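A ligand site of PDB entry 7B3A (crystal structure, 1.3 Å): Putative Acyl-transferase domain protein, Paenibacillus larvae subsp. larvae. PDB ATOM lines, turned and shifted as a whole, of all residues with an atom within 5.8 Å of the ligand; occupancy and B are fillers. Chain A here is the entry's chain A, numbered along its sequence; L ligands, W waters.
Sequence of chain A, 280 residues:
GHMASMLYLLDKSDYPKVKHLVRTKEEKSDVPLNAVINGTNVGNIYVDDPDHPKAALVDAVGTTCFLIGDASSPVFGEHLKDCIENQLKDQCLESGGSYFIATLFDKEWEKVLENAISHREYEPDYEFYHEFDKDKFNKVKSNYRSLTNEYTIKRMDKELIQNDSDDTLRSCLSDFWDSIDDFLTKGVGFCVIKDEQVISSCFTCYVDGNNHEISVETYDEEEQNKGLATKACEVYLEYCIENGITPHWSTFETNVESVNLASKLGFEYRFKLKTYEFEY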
ATOM      1  N   ARG A 145      -0.247 -22.696   8.710  1.00  0.00           N
ATOM      2  CA  ARG A 145      -0.664 -21.283   8.828  1.00  0.00           C
ATOM      3  C   ARG A 145      -1.964 -21.159   9.586  1.00  0.00           C
ATOM      4  O   ARG A 145      -2.934 -21.863   9.311  1.00  0.00           O
ATOM      5  CB  ARG A 145      -0.901 -20.693   7.433  1.00  0.00           C
ATOM      6  CG  ARG A 145      -0.756 -19.162   7.319  1.00  0.00           C
ATOM      7  CD  ARG A 145      -1.296 -18.631   5.992  1.00  0.00           C
ATOM      8  NE  ARG A 145      -0.812 -19.345   4.825  1.00  0.00           N
ATOM      9  CZ  ARG A 145      -0.116 -18.801   3.816  1.00  0.00           C
ATOM     10  NH1 ARG A 145       0.216 -17.485   3.844  1.00  0.00           N
ATOM     11  NH2 ARG A 145       0.248 -19.573   2.781  1.00  0.00           N
ATOM     12  N   SER A 200     -14.149 -23.831   2.035  1.00  0.00           N
ATOM     13  CA  SER A 200     -13.450 -25.118   1.964  1.00  0.00           C
ATOM     14  C   SER A 200     -14.195 -26.171   2.801  1.00  0.00           C
ATOM     15  O   SER A 200     -14.861 -25.855   3.784  1.00  0.00           O
ATOM     16  CB  SER A 200     -12.038 -25.040   2.559  1.00  0.00           C
ATOM     17  OG  SER A 200     -11.292 -24.020   1.907  1.00  0.00           O
ATOM     18  N   ILE A 214     -11.575 -39.499   2.858  1.00  0.00           N
ATOM     19  CA  ILE A 214     -11.662 -38.046   2.775  1.00  0.00           C
ATOM     20  C   ILE A 214     -12.070 -37.562   1.403  1.00  0.00           C
ATOM     21  O   ILE A 214     -11.552 -38.025   0.393  1.00  0.00           O
ATOM     22  CB  ILE A 214     -10.278 -37.445   3.114  1.00  0.00           C
ATOM     23  CG1 ILE A 214     -10.124 -37.521   4.624  1.00  0.00           C
ATOM     24  CG2 ILE A 214     -10.126 -36.022   2.624  1.00  0.00           C
ATOM     25  CD1 ILE A 214      -8.683 -37.279   5.077  1.00  0.00           C
ATOM     26  N   SER A 215     -12.930 -36.513   1.409  1.00  0.00           N
ATOM     27  CA  SER A 215     -13.079 -35.572   0.293  1.00  0.00           C
ATOM     28  C   SER A 215     -12.780 -34.156   0.765  1.00  0.00           C
ATOM     29  O   SER A 215     -13.337 -33.713   1.761  1.00  0.00           O
ATOM     30  CB  SER A 215     -14.508 -35.628  -0.160  1.00  0.00           C
ATOM     31  OG  SER A 215     -14.751 -34.566  -1.087  1.00  0.00           O
ATOM     32  N   VAL A 216     -11.839 -33.506   0.113  1.00  0.00           N
ATOM     33  CA  VAL A 216     -11.453 -32.126   0.416  1.00  0.00           C
ATOM     34  C   VAL A 216     -11.620 -31.266  -0.840  1.00  0.00           C
ATOM     35  O   VAL A 216     -11.300 -31.693  -1.950  1.00  0.00           O
ATOM     36  CB  VAL A 216     -10.009 -32.086   0.961  1.00  0.00           C
ATOM     37  CG1 VAL A 216      -8.984 -32.491  -0.040  1.00  0.00           C
ATOM     38  CG2 VAL A 216      -9.647 -30.678   1.502  1.00  0.00           C
ATOM     39  N   GLU A 217     -11.980 -29.996  -0.610  1.00  0.00           N
ATOM     40  CA  GLU A 217     -12.079 -29.032  -1.682  1.00  0.00           C
ATOM     41  C   GLU A 217     -12.079 -27.604  -1.128  1.00  0.00           C
ATOM     42  O   GLU A 217     -12.750 -27.334  -0.126  1.00  0.00           O
ATOM     43  CB  GLU A 217     -13.367 -29.238  -2.516  1.00  0.00           C
ATOM     44  CG  GLU A 217     -13.404 -28.358  -3.758  1.00  0.00           C
ATOM     45  CD  GLU A 217     -14.320 -28.892  -4.858  1.00  0.00           C
ATOM     46  OE1 GLU A 217     -14.983 -29.930  -4.728  1.00  0.00           O
ATOM     47  OE2 GLU A 217     -14.391 -28.232  -5.913  1.00  0.00           O
ATOM     48  N   THR A 218     -11.417 -26.681  -1.837  1.00  0.00           N
ATOM     49  CA  THR A 218     -11.604 -25.236  -1.646  1.00  0.00           C
ATOM     50  C   THR A 218     -12.330 -24.733  -2.887  1.00  0.00           C
ATOM     51  O   THR A 218     -11.802 -24.803  -4.002  1.00  0.00           O
ATOM     52  CB  THR A 218     -10.253 -24.526  -1.405  1.00  0.00           C
ATOM     53  OG1 THR A 218      -9.712 -24.989  -0.149  1.00  0.00           O
ATOM     54  CG2 THR A 218     -10.411 -23.025  -1.378  1.00  0.00           C
ATOM     55  N   TYR A 219     -13.590 -24.377  -2.664  1.00  0.00           N
ATOM     56  CA  TYR A 219     -14.559 -24.116  -3.742  1.00  0.00           C
ATOM     57  C   TYR A 219     -14.284 -22.813  -4.454  1.00  0.00           C
ATOM     58  O   TYR A 219     -14.592 -22.674  -5.633  1.00  0.00           O
ATOM     59  CB  TYR A 219     -16.007 -24.112  -3.215  1.00  0.00           C
ATOM     60  CG  TYR A 219     -16.383 -25.440  -2.568  1.00  0.00           C
ATOM     61  CD1 TYR A 219     -16.639 -26.584  -3.367  1.00  0.00           C
ATOM     62  CD2 TYR A 219     -16.479 -25.583  -1.183  1.00  0.00           C
ATOM     63  CE1 TYR A 219     -16.943 -27.749  -2.818  1.00  0.00           C
ATOM     64  CE2 TYR A 219     -16.804 -26.838  -0.609  1.00  0.00           C
ATOM     65  CZ  TYR A 219     -17.039 -27.892  -1.433  1.00  0.00           C
ATOM     66  OH  TYR A 219     -17.323 -29.153  -0.856  1.00  0.00           O
ATOM     67  N   GLU A 223      -9.473 -18.303  -3.327  1.00  0.00           N
ATOM     68  CA  GLU A 223      -9.070 -18.509  -1.937  1.00  0.00           C
ATOM     69  C   GLU A 223      -8.147 -19.721  -1.747  1.00  0.00           C
ATOM     70  O   GLU A 223      -7.801 -20.075  -0.600  1.00  0.00           O
ATOM     71  CB  GLU A 223     -10.313 -18.748  -1.074  1.00  0.00           C
ATOM     72  CG  GLU A 223     -11.245 -17.553  -1.009  1.00  0.00           C
ATOM     73  CD  GLU A 223     -10.811 -16.513  -0.006  1.00  0.00           C
ATOM     74  OE1 GLU A 223      -9.642 -16.484   0.425  1.00  0.00           O
ATOM     75  OE2 GLU A 223     -11.657 -15.697   0.332  1.00  0.00           O
ATOM     76  N   GLN A 224      -7.739 -20.339  -2.845  1.00  0.00           N
ATOM     77  CA  GLN A 224      -6.790 -21.434  -2.746  1.00  0.00           C
ATOM     78  C   GLN A 224      -5.391 -20.897  -2.435  1.00  0.00           C
ATOM     79  O   GLN A 224      -5.085 -19.728  -2.629  1.00  0.00           O
ATOM     80  CB  GLN A 224      -6.805 -22.239  -4.060  1.00  0.00           C
ATOM     81  CG  GLN A 224      -8.143 -22.949  -4.225  1.00  0.00           C
ATOM     82  CD  GLN A 224      -8.259 -23.738  -5.524  1.00  0.00           C
ATOM     83  OE1 GLN A 224      -7.398 -23.634  -6.429  1.00  0.00           O
ATOM     84  NE2 GLN A 224      -9.293 -24.545  -5.607  1.00  0.00           N
ATOM     85  N   ASN A 225      -4.546 -21.794  -1.931  1.00  0.00           N
ATOM     86  CA  ASN A 225      -3.157 -21.470  -1.608  1.00  0.00           C
ATOM     87  C   ASN A 225      -3.023 -20.501  -0.458  1.00  0.00           C
ATOM     88  O   ASN A 225      -2.056 -19.727  -0.384  1.00  0.00           O
ATOM     89  CB  ASN A 225      -2.394 -20.971  -2.825  1.00  0.00           C
ATOM     90  CG  ASN A 225      -2.585 -21.858  -3.944  1.00  0.00           C
ATOM     91  OD1 ASN A 225      -2.168 -22.979  -3.877  1.00  0.00           O
ATOM     92  ND2 ASN A 225      -3.240 -21.400  -4.993  1.00  0.00           N
ATOM     93  N   LYS A 226      -3.979 -20.544   0.465  1.00  0.00           N
ATOM     94  CA  LYS A 226      -3.953 -19.695   1.642  1.00  0.00           C
ATOM     95  C   LYS A 226      -3.942 -20.487   2.946  1.00  0.00           C
ATOM     96  O   LYS A 226      -3.915 -19.909   4.017  1.00  0.00           O
ATOM     97  CB  LYS A 226      -5.132 -18.690   1.623  1.00  0.00           C
ATOM     98  CG  LYS A 226      -4.980 -17.602   0.577  1.00  0.00           C
ATOM     99  CD  LYS A 226      -6.119 -16.549   0.667  1.00  0.00           C
ATOM    100  CE  LYS A 226      -5.956 -15.500  -0.427  1.00  0.00           C
ATOM    101  NZ  LYS A 226      -7.219 -14.955  -0.886  1.00  0.00           N
ATOM    102  N   GLY A 227      -3.932 -21.811   2.890  1.00  0.00           N
ATOM    103  CA  GLY A 227      -3.974 -22.618   4.091  1.00  0.00           C
ATOM    104  C   GLY A 227      -5.365 -23.044   4.534  1.00  0.00           C
ATOM    105  O   GLY A 227      -5.488 -23.680   5.591  1.00  0.00           O
ATOM    106  N   LEU A 228      -6.396 -22.765   3.730  1.00  0.00           N
ATOM    107  CA  LEU A 228      -7.770 -23.060   4.141  1.00  0.00           C
ATOM    108  C   LEU A 228      -8.106 -24.552   4.109  1.00  0.00           C
ATOM    109  O   LEU A 228      -8.652 -25.090   5.094  1.00  0.00           O
ATOM    110  CB  LEU A 228      -8.744 -22.219   3.292  1.00  0.00           C
ATOM    111  CG  LEU A 228      -8.472 -20.719   3.255  1.00  0.00           C
ATOM    112  CD1 LEU A 228      -9.625 -20.041   2.559  1.00  0.00           C
ATOM    113  CD2 LEU A 228      -8.261 -20.146   4.663  1.00  0.00           C
ATOM    114  N   ALA A 229      -7.802 -25.234   3.016  1.00  0.00           N
ATOM    115  CA  ALA A 229      -8.040 -26.672   3.038  1.00  0.00           C
ATOM    116  C   ALA A 229      -7.224 -27.348   4.122  1.00  0.00           C
ATOM    117  O   ALA A 229      -7.696 -28.284   4.772  1.00  0.00           O
ATOM    118  CB  ALA A 229      -7.791 -27.306   1.676  1.00  0.00           C
ATOM    119  N   THR A 230      -6.000 -26.921   4.316  1.00  0.00           N
ATOM    120  CA  THR A 230      -5.175 -27.484   5.354  1.00  0.00           C
ATOM    121  C   THR A 230      -5.856 -27.397   6.711  1.00  0.00           C
ATOM    122  O   THR A 230      -5.859 -28.365   7.481  1.00  0.00           O
ATOM    123  CB  THR A 230      -3.825 -26.734   5.427  1.00  0.00           C
ATOM    124  OG1 THR A 230      -3.064 -26.976   4.230  1.00  0.00           O
ATOM    125  CG2 THR A 230      -3.006 -27.199   6.577  1.00  0.00           C
ATOM    126  N   LYS A 231      -6.464 -26.246   7.010  1.00  0.00           N
ATOM    127  CA  LYS A 231      -7.070 -26.113   8.326  1.00  0.00           C
ATOM    128  C   LYS A 231      -8.350 -26.899   8.440  1.00  0.00           C
ATOM    129  O   LYS A 231      -8.640 -27.461   9.510  1.00  0.00           O
ATOM    130  CB  LYS A 231      -7.313 -24.646   8.691  1.00  0.00           C
ATOM    131  CG  LYS A 231      -6.048 -23.925   9.090  1.00  0.00           C
ATOM    132  CD  LYS A 231      -5.200 -24.621  10.171  1.00  0.00           C
ATOM    133  CE  LYS A 231      -5.492 -24.153  11.589  1.00  0.00           C
ATOM    134  NZ  LYS A 231      -4.283 -24.252  12.493  1.00  0.00           N
ATOM    135  N   HIS A 248      -8.425 -41.925   5.321  1.00  0.00           N
ATOM    136  CA  HIS A 248      -7.771 -42.325   4.081  1.00  0.00           C
ATOM    137  C   HIS A 248      -7.859 -41.253   3.031  1.00  0.00           C
ATOM    138  O   HIS A 248      -8.891 -40.583   2.899  1.00  0.00           O
ATOM    139  CB  HIS A 248      -8.411 -43.574   3.498  1.00  0.00           C
ATOM    140  CG  HIS A 248      -8.336 -44.803   4.353  1.00  0.00           C
ATOM    141  ND1 HIS A 248      -7.724 -45.956   3.914  1.00  0.00           N
ATOM    142  CD2 HIS A 248      -8.807 -45.071   5.605  1.00  0.00           C
ATOM    143  CE1 HIS A 248      -7.813 -46.891   4.866  1.00  0.00           C
ATOM    144  NE2 HIS A 248      -8.484 -46.385   5.890  1.00  0.00           N
ATOM    145  N   TRP A 249      -6.748 -41.058   2.336  1.00  0.00           N
ATOM    146  CA  TRP A 249      -6.617 -40.081   1.260  1.00  0.00           C
ATOM    147  C   TRP A 249      -6.134 -40.803   0.021  1.00  0.00           C
ATOM    148  O   TRP A 249      -5.035 -41.382   0.040  1.00  0.00           O
ATOM    149  CB  TRP A 249      -5.456 -39.111   1.633  1.00  0.00           C
ATOM    150  CG  TRP A 249      -5.334 -37.831   0.800  1.00  0.00           C
ATOM    151  CD1 TRP A 249      -4.984 -37.694  -0.507  1.00  0.00           C
ATOM    152  CD2 TRP A 249      -5.650 -36.510   1.279  1.00  0.00           C
ATOM    153  NE1 TRP A 249      -5.051 -36.359  -0.887  1.00  0.00           N
ATOM    154  CE2 TRP A 249      -5.430 -35.617   0.215  1.00  0.00           C
ATOM    155  CE3 TRP A 249      -6.062 -36.011   2.511  1.00  0.00           C
ATOM    156  CZ2 TRP A 249      -5.654 -34.233   0.344  1.00  0.00           C
ATOM    157  CZ3 TRP A 249      -6.304 -34.634   2.654  1.00  0.00           C
ATOM    158  CH2 TRP A 249      -6.042 -33.776   1.572  1.00  0.00           C
ATOM    159  N   SER A 250      -6.893 -40.741  -1.041  1.00  0.00           N
ATOM    160  CA  SER A 250      -6.512 -41.353  -2.303  1.00  0.00           C
ATOM    161  C   SER A 250      -6.710 -40.290  -3.371  1.00  0.00           C
ATOM    162  O   SER A 250      -7.692 -39.547  -3.338  1.00  0.00           O
ATOM    163  CB  SER A 250      -7.373 -42.588  -2.579  1.00  0.00           C
ATOM    164  OG  SER A 250      -7.390 -43.446  -1.400  1.00  0.00           O
ATOM    165  N   THR A 251      -5.762 -40.146  -4.282  1.00  0.00           N
ATOM    166  CA  THR A 251      -5.889 -39.060  -5.262  1.00  0.00           C
ATOM    167  C   THR A 251      -5.152 -39.397  -6.528  1.00  0.00           C
ATOM    168  O   THR A 251      -4.186 -40.156  -6.490  1.00  0.00           O
ATOM    169  CB  THR A 251      -5.406 -37.736  -4.666  1.00  0.00           C
ATOM    170  OG1 THR A 251      -5.852 -36.620  -5.486  1.00  0.00           O
ATOM    171  CG2 THR A 251      -3.896 -37.704  -4.507  1.00  0.00           C
ATOM    172  N   PHE A 252      -5.609 -38.817  -7.649  1.00  0.00           N
ATOM    173  CA  PHE A 252      -4.903 -39.030  -8.922  1.00  0.00           C
ATOM    174  C   PHE A 252      -3.486 -38.473  -8.889  1.00  0.00           C
ATOM    175  O   PHE A 252      -3.234 -37.395  -8.355  1.00  0.00           O
ATOM    176  CB  PHE A 252      -5.584 -38.326 -10.082  1.00  0.00           C
ATOM    177  CG  PHE A 252      -6.885 -38.924 -10.595  1.00  0.00           C
ATOM    178  CD1 PHE A 252      -6.947 -40.211 -11.131  1.00  0.00           C
ATOM    179  CD2 PHE A 252      -8.038 -38.126 -10.703  1.00  0.00           C
ATOM    180  CE1 PHE A 252      -8.127 -40.710 -11.673  1.00  0.00           C
ATOM    181  CE2 PHE A 252      -9.209 -38.630 -11.287  1.00  0.00           C
ATOM    182  CZ  PHE A 252      -9.268 -39.922 -11.755  1.00  0.00           C
ATOM    183  N   ASN A 255      -3.119 -35.041  -9.936  1.00  0.00           N
ATOM    184  CA  ASN A 255      -3.669 -33.972  -9.108  1.00  0.00           C
ATOM    185  C   ASN A 255      -2.612 -33.573  -8.082  1.00  0.00           C
ATOM    186  O   ASN A 255      -2.654 -33.957  -6.934  1.00  0.00           O
ATOM    187  CB  ASN A 255      -4.958 -34.446  -8.462  1.00  0.00           C
ATOM    188  CG  ASN A 255      -5.693 -33.375  -7.742  1.00  0.00           C
ATOM    189  OD1 ASN A 255      -5.155 -32.314  -7.407  1.00  0.00           O
ATOM    190  ND2 ASN A 255      -6.908 -33.683  -7.402  1.00  0.00           N
ATOM    191  N   VAL A 256      -1.583 -32.826  -8.547  1.00  0.00           N
ATOM    192  CA  VAL A 256      -0.420 -32.658  -7.665  1.00  0.00           C
ATOM    193  C   VAL A 256      -0.742 -31.753  -6.500  1.00  0.00           C
ATOM    194  O   VAL A 256      -0.071 -31.852  -5.478  1.00  0.00           O
ATOM    195  CB  VAL A 256       0.892 -32.222  -8.328  1.00  0.00           C
ATOM    196  CG1 VAL A 256       1.338 -33.253  -9.410  1.00  0.00           C
ATOM    197  CG2 VAL A 256       0.722 -30.943  -8.901  1.00  0.00           C
ATOM    198  N   GLU A 257      -1.779 -30.897  -6.600  1.00  0.00           N
ATOM    199  CA  GLU A 257      -2.169 -30.108  -5.409  1.00  0.00           C
ATOM    200  C   GLU A 257      -2.615 -31.032  -4.279  1.00  0.00           C
ATOM    201  O   GLU A 257      -2.215 -30.860  -3.107  1.00  0.00           O
ATOM    202  CB  GLU A 257      -3.296 -29.130  -5.720  1.00  0.00           C
ATOM    203  CG  GLU A 257      -3.015 -28.041  -6.798  1.00  0.00           C
ATOM    204  CD  GLU A 257      -3.384 -28.436  -8.235  1.00  0.00           C
ATOM    205  OE1 GLU A 257      -3.674 -29.640  -8.481  1.00  0.00           O
ATOM    206  OE2 GLU A 257      -3.351 -27.520  -9.114  1.00  0.00           O
ATOM    207  N   SER A 258      -3.357 -32.064  -4.648  1.00  0.00           N
ATOM    208  CA  SER A 258      -3.843 -33.045  -3.678  1.00  0.00           C
ATOM    209  C   SER A 258      -2.742 -34.014  -3.230  1.00  0.00           C
ATOM    210  O   SER A 258      -2.652 -34.291  -2.039  1.00  0.00           O
ATOM    211  CB  SER A 258      -5.025 -33.768  -4.291  1.00  0.00           C
ATOM    212  OG  SER A 258      -5.489 -34.675  -3.329  1.00  0.00           O
ATOM    213  N   ASN A 260       0.416 -33.289  -2.974  1.00  0.00           N
ATOM    214  CA  ASN A 260       1.264 -32.525  -2.064  1.00  0.00           C
ATOM    215  C   ASN A 260       0.554 -32.248  -0.741  1.00  0.00           C
ATOM    216  O   ASN A 260       1.175 -32.344   0.302  1.00  0.00           O
ATOM    217  CB  ASN A 260       1.710 -31.199  -2.710  1.00  0.00           C
ATOM    218  CG  ASN A 260       2.756 -31.409  -3.747  1.00  0.00           C
ATOM    219  OD1 ASN A 260       3.757 -32.025  -3.497  1.00  0.00           O
ATOM    220  ND2 ASN A 260       2.562 -30.846  -4.871  1.00  0.00           N
ATOM    221  N   LEU A 261      -0.752 -31.939  -0.781  1.00  0.00           N
ATOM    222  CA  LEU A 261      -1.492 -31.695   0.469  1.00  0.00           C
ATOM    223  C   LEU A 261      -1.503 -32.963   1.329  1.00  0.00           C
ATOM    224  O   LEU A 261      -1.332 -32.902   2.557  1.00  0.00           O
ATOM    225  CB  LEU A 261      -2.862 -31.142   0.137  1.00  0.00           C
ATOM    226  CG  LEU A 261      -3.729 -30.937   1.381  1.00  0.00           C
ATOM    227  CD1 LEU A 261      -3.033 -29.998   2.414  1.00  0.00           C
ATOM    228  CD2 LEU A 261      -5.101 -30.364   1.019  1.00  0.00           C
ATOM    229  N   LYS A 264       1.684 -33.132   3.115  1.00  0.00           N
ATOM    230  CA  LYS A 264       1.732 -32.140   4.158  1.00  0.00           C
ATOM    231  C   LYS A 264       0.983 -32.556   5.416  1.00  0.00           C
ATOM    232  O   LYS A 264       1.377 -32.128   6.527  1.00  0.00           O
ATOM    233  CB  LYS A 264       1.158 -30.839   3.587  1.00  0.00           C
ATOM    234  CG  LYS A 264       1.051 -29.704   4.594  1.00  0.00           C
ATOM    235  CD  LYS A 264       0.468 -28.442   3.930  1.00  0.00           C
ATOM    236  CE  LYS A 264       0.387 -27.277   4.925  1.00  0.00           C
ATOM    237  NZ  LYS A 264      -0.385 -26.123   4.338  1.00  0.00           N
HETATM  238  N1  LIG L   1       1.038 -26.918  -6.628  1.00  0.00           N
HETATM  239  C1  LIG L   1       1.547 -27.837  -5.769  1.00  0.00           C
HETATM  240  N2  LIG L   1       0.993 -28.090  -4.533  1.00  0.00           N
HETATM  241  C2  LIG L   1      -0.060 -27.319  -4.199  1.00  0.00           C
HETATM  242  C3  LIG L   1      -0.598 -26.407  -5.044  1.00  0.00           C
HETATM  243  C4  LIG L   1       0.000 -26.197  -6.262  1.00  0.00           C
HETATM  244  N3  LIG L   1      -0.210 -25.363  -7.410  1.00  0.00           N
HETATM  245  N4  LIG L   1      -1.672 -25.842  -4.410  1.00  0.00           N
HETATM  246  C5  LIG L   1      -1.814 -26.433  -3.209  1.00  0.00           C
HETATM  247  N5  LIG L   1      -0.788 -27.358  -3.060  1.00  0.00           N
HETATM  248  C6  LIG L   1      -0.476 -28.217  -1.946  1.00  0.00           C
HETATM  249  C7  LIG L   1       0.715 -27.894  -1.278  1.00  0.00           C
HETATM  250  O1  LIG L   1       1.062 -29.013  -0.414  1.00  0.00           O
HETATM  251  C8  LIG L   1       0.471 -26.729  -0.348  1.00  0.00           C
HETATM  252  O2  LIG L   1       1.354 -26.733   0.690  1.00  0.00           O
HETATM  253  P1  LIG L   1       1.785 -25.330   1.416  1.00  0.00           P
HETATM  254  O3  LIG L   1       3.047 -25.757   2.140  1.00  0.00           O
HETATM  255  O4  LIG L   1       2.160 -24.406   0.307  1.00  0.00           O
HETATM  256  O5  LIG L   1       0.688 -24.854   2.291  1.00  0.00           O
HETATM  257  C9  LIG L   1      -0.978 -27.071   0.104  1.00  0.00           C
HETATM  258  O6  LIG L   1      -1.511 -27.869  -0.814  1.00  0.00           O
HETATM  259  C10 LIG L   1      -1.717 -25.705   0.110  1.00  0.00           C
HETATM  260  O7  LIG L   1      -2.635 -25.928   1.086  1.00  0.00           O
HETATM  261  P2  LIG L   1      -3.987 -25.096   1.115  1.00  0.00           P
HETATM  262  O8  LIG L   1      -3.691 -23.677   0.712  1.00  0.00           O
HETATM  263  O9  LIG L   1      -4.546 -25.353   2.449  1.00  0.00           O
HETATM  264  O10 LIG L   1      -4.915 -25.826   0.019  1.00  0.00           O
HETATM  265  P3  LIG L   1      -6.038 -25.136  -0.898  1.00  0.00           P
HETATM  266  O11 LIG L   1      -7.022 -24.365  -0.046  1.00  0.00           O
HETATM  267  O12 LIG L   1      -5.420 -24.441  -2.022  1.00  0.00           O
HETATM  268  O13 LIG L   1      -6.832 -26.427  -1.410  1.00  0.00           O
HETATM  269  C11 LIG L   1      -7.152 -28.425  -2.801  1.00  0.00           C
HETATM  270  C12 LIG L   1      -6.154 -27.575  -1.959  1.00  0.00           C
HETATM  271  C13 LIG L   1      -8.264 -28.850  -1.895  1.00  0.00           C
HETATM  272  C14 LIG L   1      -6.390 -29.692  -3.291  1.00  0.00           C
HETATM  273  C15 LIG L   1      -7.680 -27.512  -3.938  1.00  0.00           C
HETATM  274  O14 LIG L   1      -6.673 -27.411  -4.972  1.00  0.00           O
HETATM  275  C16 LIG L   1      -8.981 -28.031  -4.526  1.00  0.00           C
HETATM  276  O15 LIG L   1     -10.064 -27.768  -4.072  1.00  0.00           O
HETATM  277  N6  LIG L   1      -8.820 -28.845  -5.718  1.00  0.00           N
HETATM  278  C17 LIG L   1     -10.075 -29.325  -6.354  1.00  0.00           C
HETATM  279  C18 LIG L   1     -10.746 -30.462  -5.612  1.00  0.00           C
HETATM  280  C19 LIG L   1      -9.771 -31.630  -5.515  1.00  0.00           C
HETATM  281  O16 LIG L   1      -9.132 -32.074  -6.458  1.00  0.00           O
HETATM  282  N7  LIG L   1      -9.692 -32.178  -4.214  1.00  0.00           N
HETATM  283  C20 LIG L   1      -8.817 -33.363  -3.917  1.00  0.00           C
HETATM  284  C21 LIG L   1      -9.491 -34.652  -4.429  1.00  0.00           C
HETATM  285  S1  LIG L   1      -8.777 -36.105  -3.710  1.00  0.00           S
HETATM  286  C22 LIG L   1      -9.345 -36.025  -2.027  1.00  0.00           C
HETATM  287  O17 LIG L   1     -10.249 -35.256  -1.735  1.00  0.00           O
HETATM  288  C23 LIG L   1      -8.579 -36.828  -0.999  1.00  0.00           C
HETATM  289  O   HOH W   1       2.338 -22.971   4.570  1.00  0.00           O
HETATM  290  O   HOH W   2       0.133 -23.617  -2.237  1.00  0.00           O
HETATM  291  O   HOH W   3      -6.578 -29.954  -7.361  1.00  0.00           O
HETATM  292  O   HOH W   4      -1.081 -22.827   1.101  1.00  0.00           O
HETATM  293  O   HOH W   5      -9.641 -39.905  -0.711  1.00  0.00           O
HETATM  294  O   HOH W   6     -10.081 -32.291  -8.744  1.00  0.00           O
HETATM  295  O   HOH W   7       2.199 -21.726   0.967  1.00  0.00           O
HETATM  296  O   HOH W   8      -0.378 -22.204   3.999  1.00  0.00           O
HETATM  297  O   HOH W   9      -6.412 -21.922   0.787  1.00  0.00           O
HETATM  298  O   HOH W  10      -4.807 -25.340  -4.506  1.00  0.00           O
HETATM  299  O   HOH W  11      -6.819 -26.270  -7.680  1.00  0.00           O
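NZ of Lys 264 is in hydrogen-bond range of OG1 of Thr 230 (2.8 Å). The side-chain amide nitrogen (NE2) of Gln 224 is in hydrogen-bond range of the backbone carbonyl oxygen (O) of Thr 218. The side-chain carboxylate of Glu 257 sits close to the side-chain amide oxygen of Asn 255, at 3.2 Å. N of Ser 258 is in hydrogen-bond range of OD1 of Asn 255 (3.3 Å). OE1 of Glu 223 lies within salt-bridge range of NZ of Lys 226 (3.2 Å). The guanidinium group (NE) of Arg 145 lies within hydrogen-bond range of the backbone carbonyl oxygen (O) of Lys 226, at 3.3 Å. OG of Ser 258 sits at hydrogen-bond distance from OG1 of Thr 251 (2.9 Å). NE1 of Trp 249 lies within hydrogen-bond range of OG of Ser 258 (3.0 Å).
The backbone carbonyl oxygen of Ser 250 lies close to a sulfur (S1) of the ligand (3.6 Å). O of Ile 214 touches C23 of the ligand, 3.5 Å away. CA of Ser 215 touches O17 of the ligand (3.5 Å). Glu 217 touches the ligand (CA to O15, 3.4 Å). Gln 224 touches the ligand (CB to O12, 3.3 Å). NE1 of Trp 249 touches C23 of the ligand (3.6 Å). Glu 257 touches the ligand (O to C6, 3.4 Å). Hydrophobic or aromatic side chains that line the ligand: Val 216, Ala 229, Trp 249 and Leu 261. Of the 29 residues printed, 21 come within 4 Å of the ligand.
Water W7 bridges O4 of the ligand (2.8 Å) and NH2 of Arg 145 (3.4 Å). Water W11 lies within hydrogen-bond range of an oxygen (O14) of the ligand and the side-chain amide oxygen (OE1) of Gln 224. Water W3 lies within hydrogen-bond range of the side-chain amide oxygen of Asn 255, a nitrogen (N6) of the ligand and the side-chain carboxylate of Glu 257. Water W5 lies within hydrogen-bond range of the backbone NH of Ser 250 (2.9 Å) and the backbone carbonyl oxygen of Ile 214 (2.9 Å). Water W8 lies within hydrogen-bond range of the guanidinium group of Arg 145 (3.0 Å) and an oxygen (O5) of the ligand (3.3 Å). Water W2 lies within hydrogen-bond range of the side-chain amide oxygen (OD1) of Asn 225 (2.9 Å) and an oxygen (O4) of the ligand (3.3 Å).
The side-chain amino group of Lys 264 lies within salt-bridge range of an oxygen (O5) of the ligand (2.6 Å). N of Thr 218 lies within hydrogen-bond range of O15 of the ligand (2.8 Å). O11 of the ligand lies within hydrogen-bond range of OG1 of Thr 218, at 2.8 Å. O12 of the ligand lies within hydrogen-bond range of N of Asn 225 (2.8 Å). A nitrogen (N4) of the ligand lies close to the side-chain amide oxygen of Asn 225. O17 of the ligand is in hydrogen-bond range of N of Val 216 (3.0 Å). A nitrogen (N7) of the ligand sits at hydrogen-bond distance from the backbone carbonyl oxygen of Val 216 (2.8 Å). The backbone NH of Thr 230 is in hydrogen-bond range of an oxygen (O9) of the ligand (2.8 Å). An oxygen (O9) of the ligand is in hydrogen-bond range of the side-chain hydroxyl of Thr 230. An oxygen (O8) of the ligand lies within hydrogen-bond range of the backbone NH (N) of Gly 227, at 2.9 Å. An oxygen (O16) of the ligand is in hydrogen-bond range of the side-chain amide nitrogen of Asn 255, at 2.9 Å. N of Lys 226 is in hydrogen-bond range of O8 of the ligand (3.2 Å). The backbone carbonyl oxygen (O) of Asn 260 sits close to an oxygen (O1) of the ligand (3.4 Å). A nitrogen (N2) of the ligand lies within hydrogen-bond range of the side-chain amide nitrogen (ND2) of Asn 260 (3.2 Å). The backbone NH (N) of Ala 229 is in hydrogen-bond range of an oxygen (O11) of the ligand. An oxygen (O9) of the ligand is in hydrogen-bond range of the backbone NH (N) of Leu 228 (3.4 Å). OG1 of Thr 251 sits close to S1 of the ligand (3.5 Å). N of Leu 261 is in hydrogen-bond range of O1 of the ligand, at 3.5 Å. OG of Ser 258 lies close to S1 of the ligand, at 3.6 Å.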
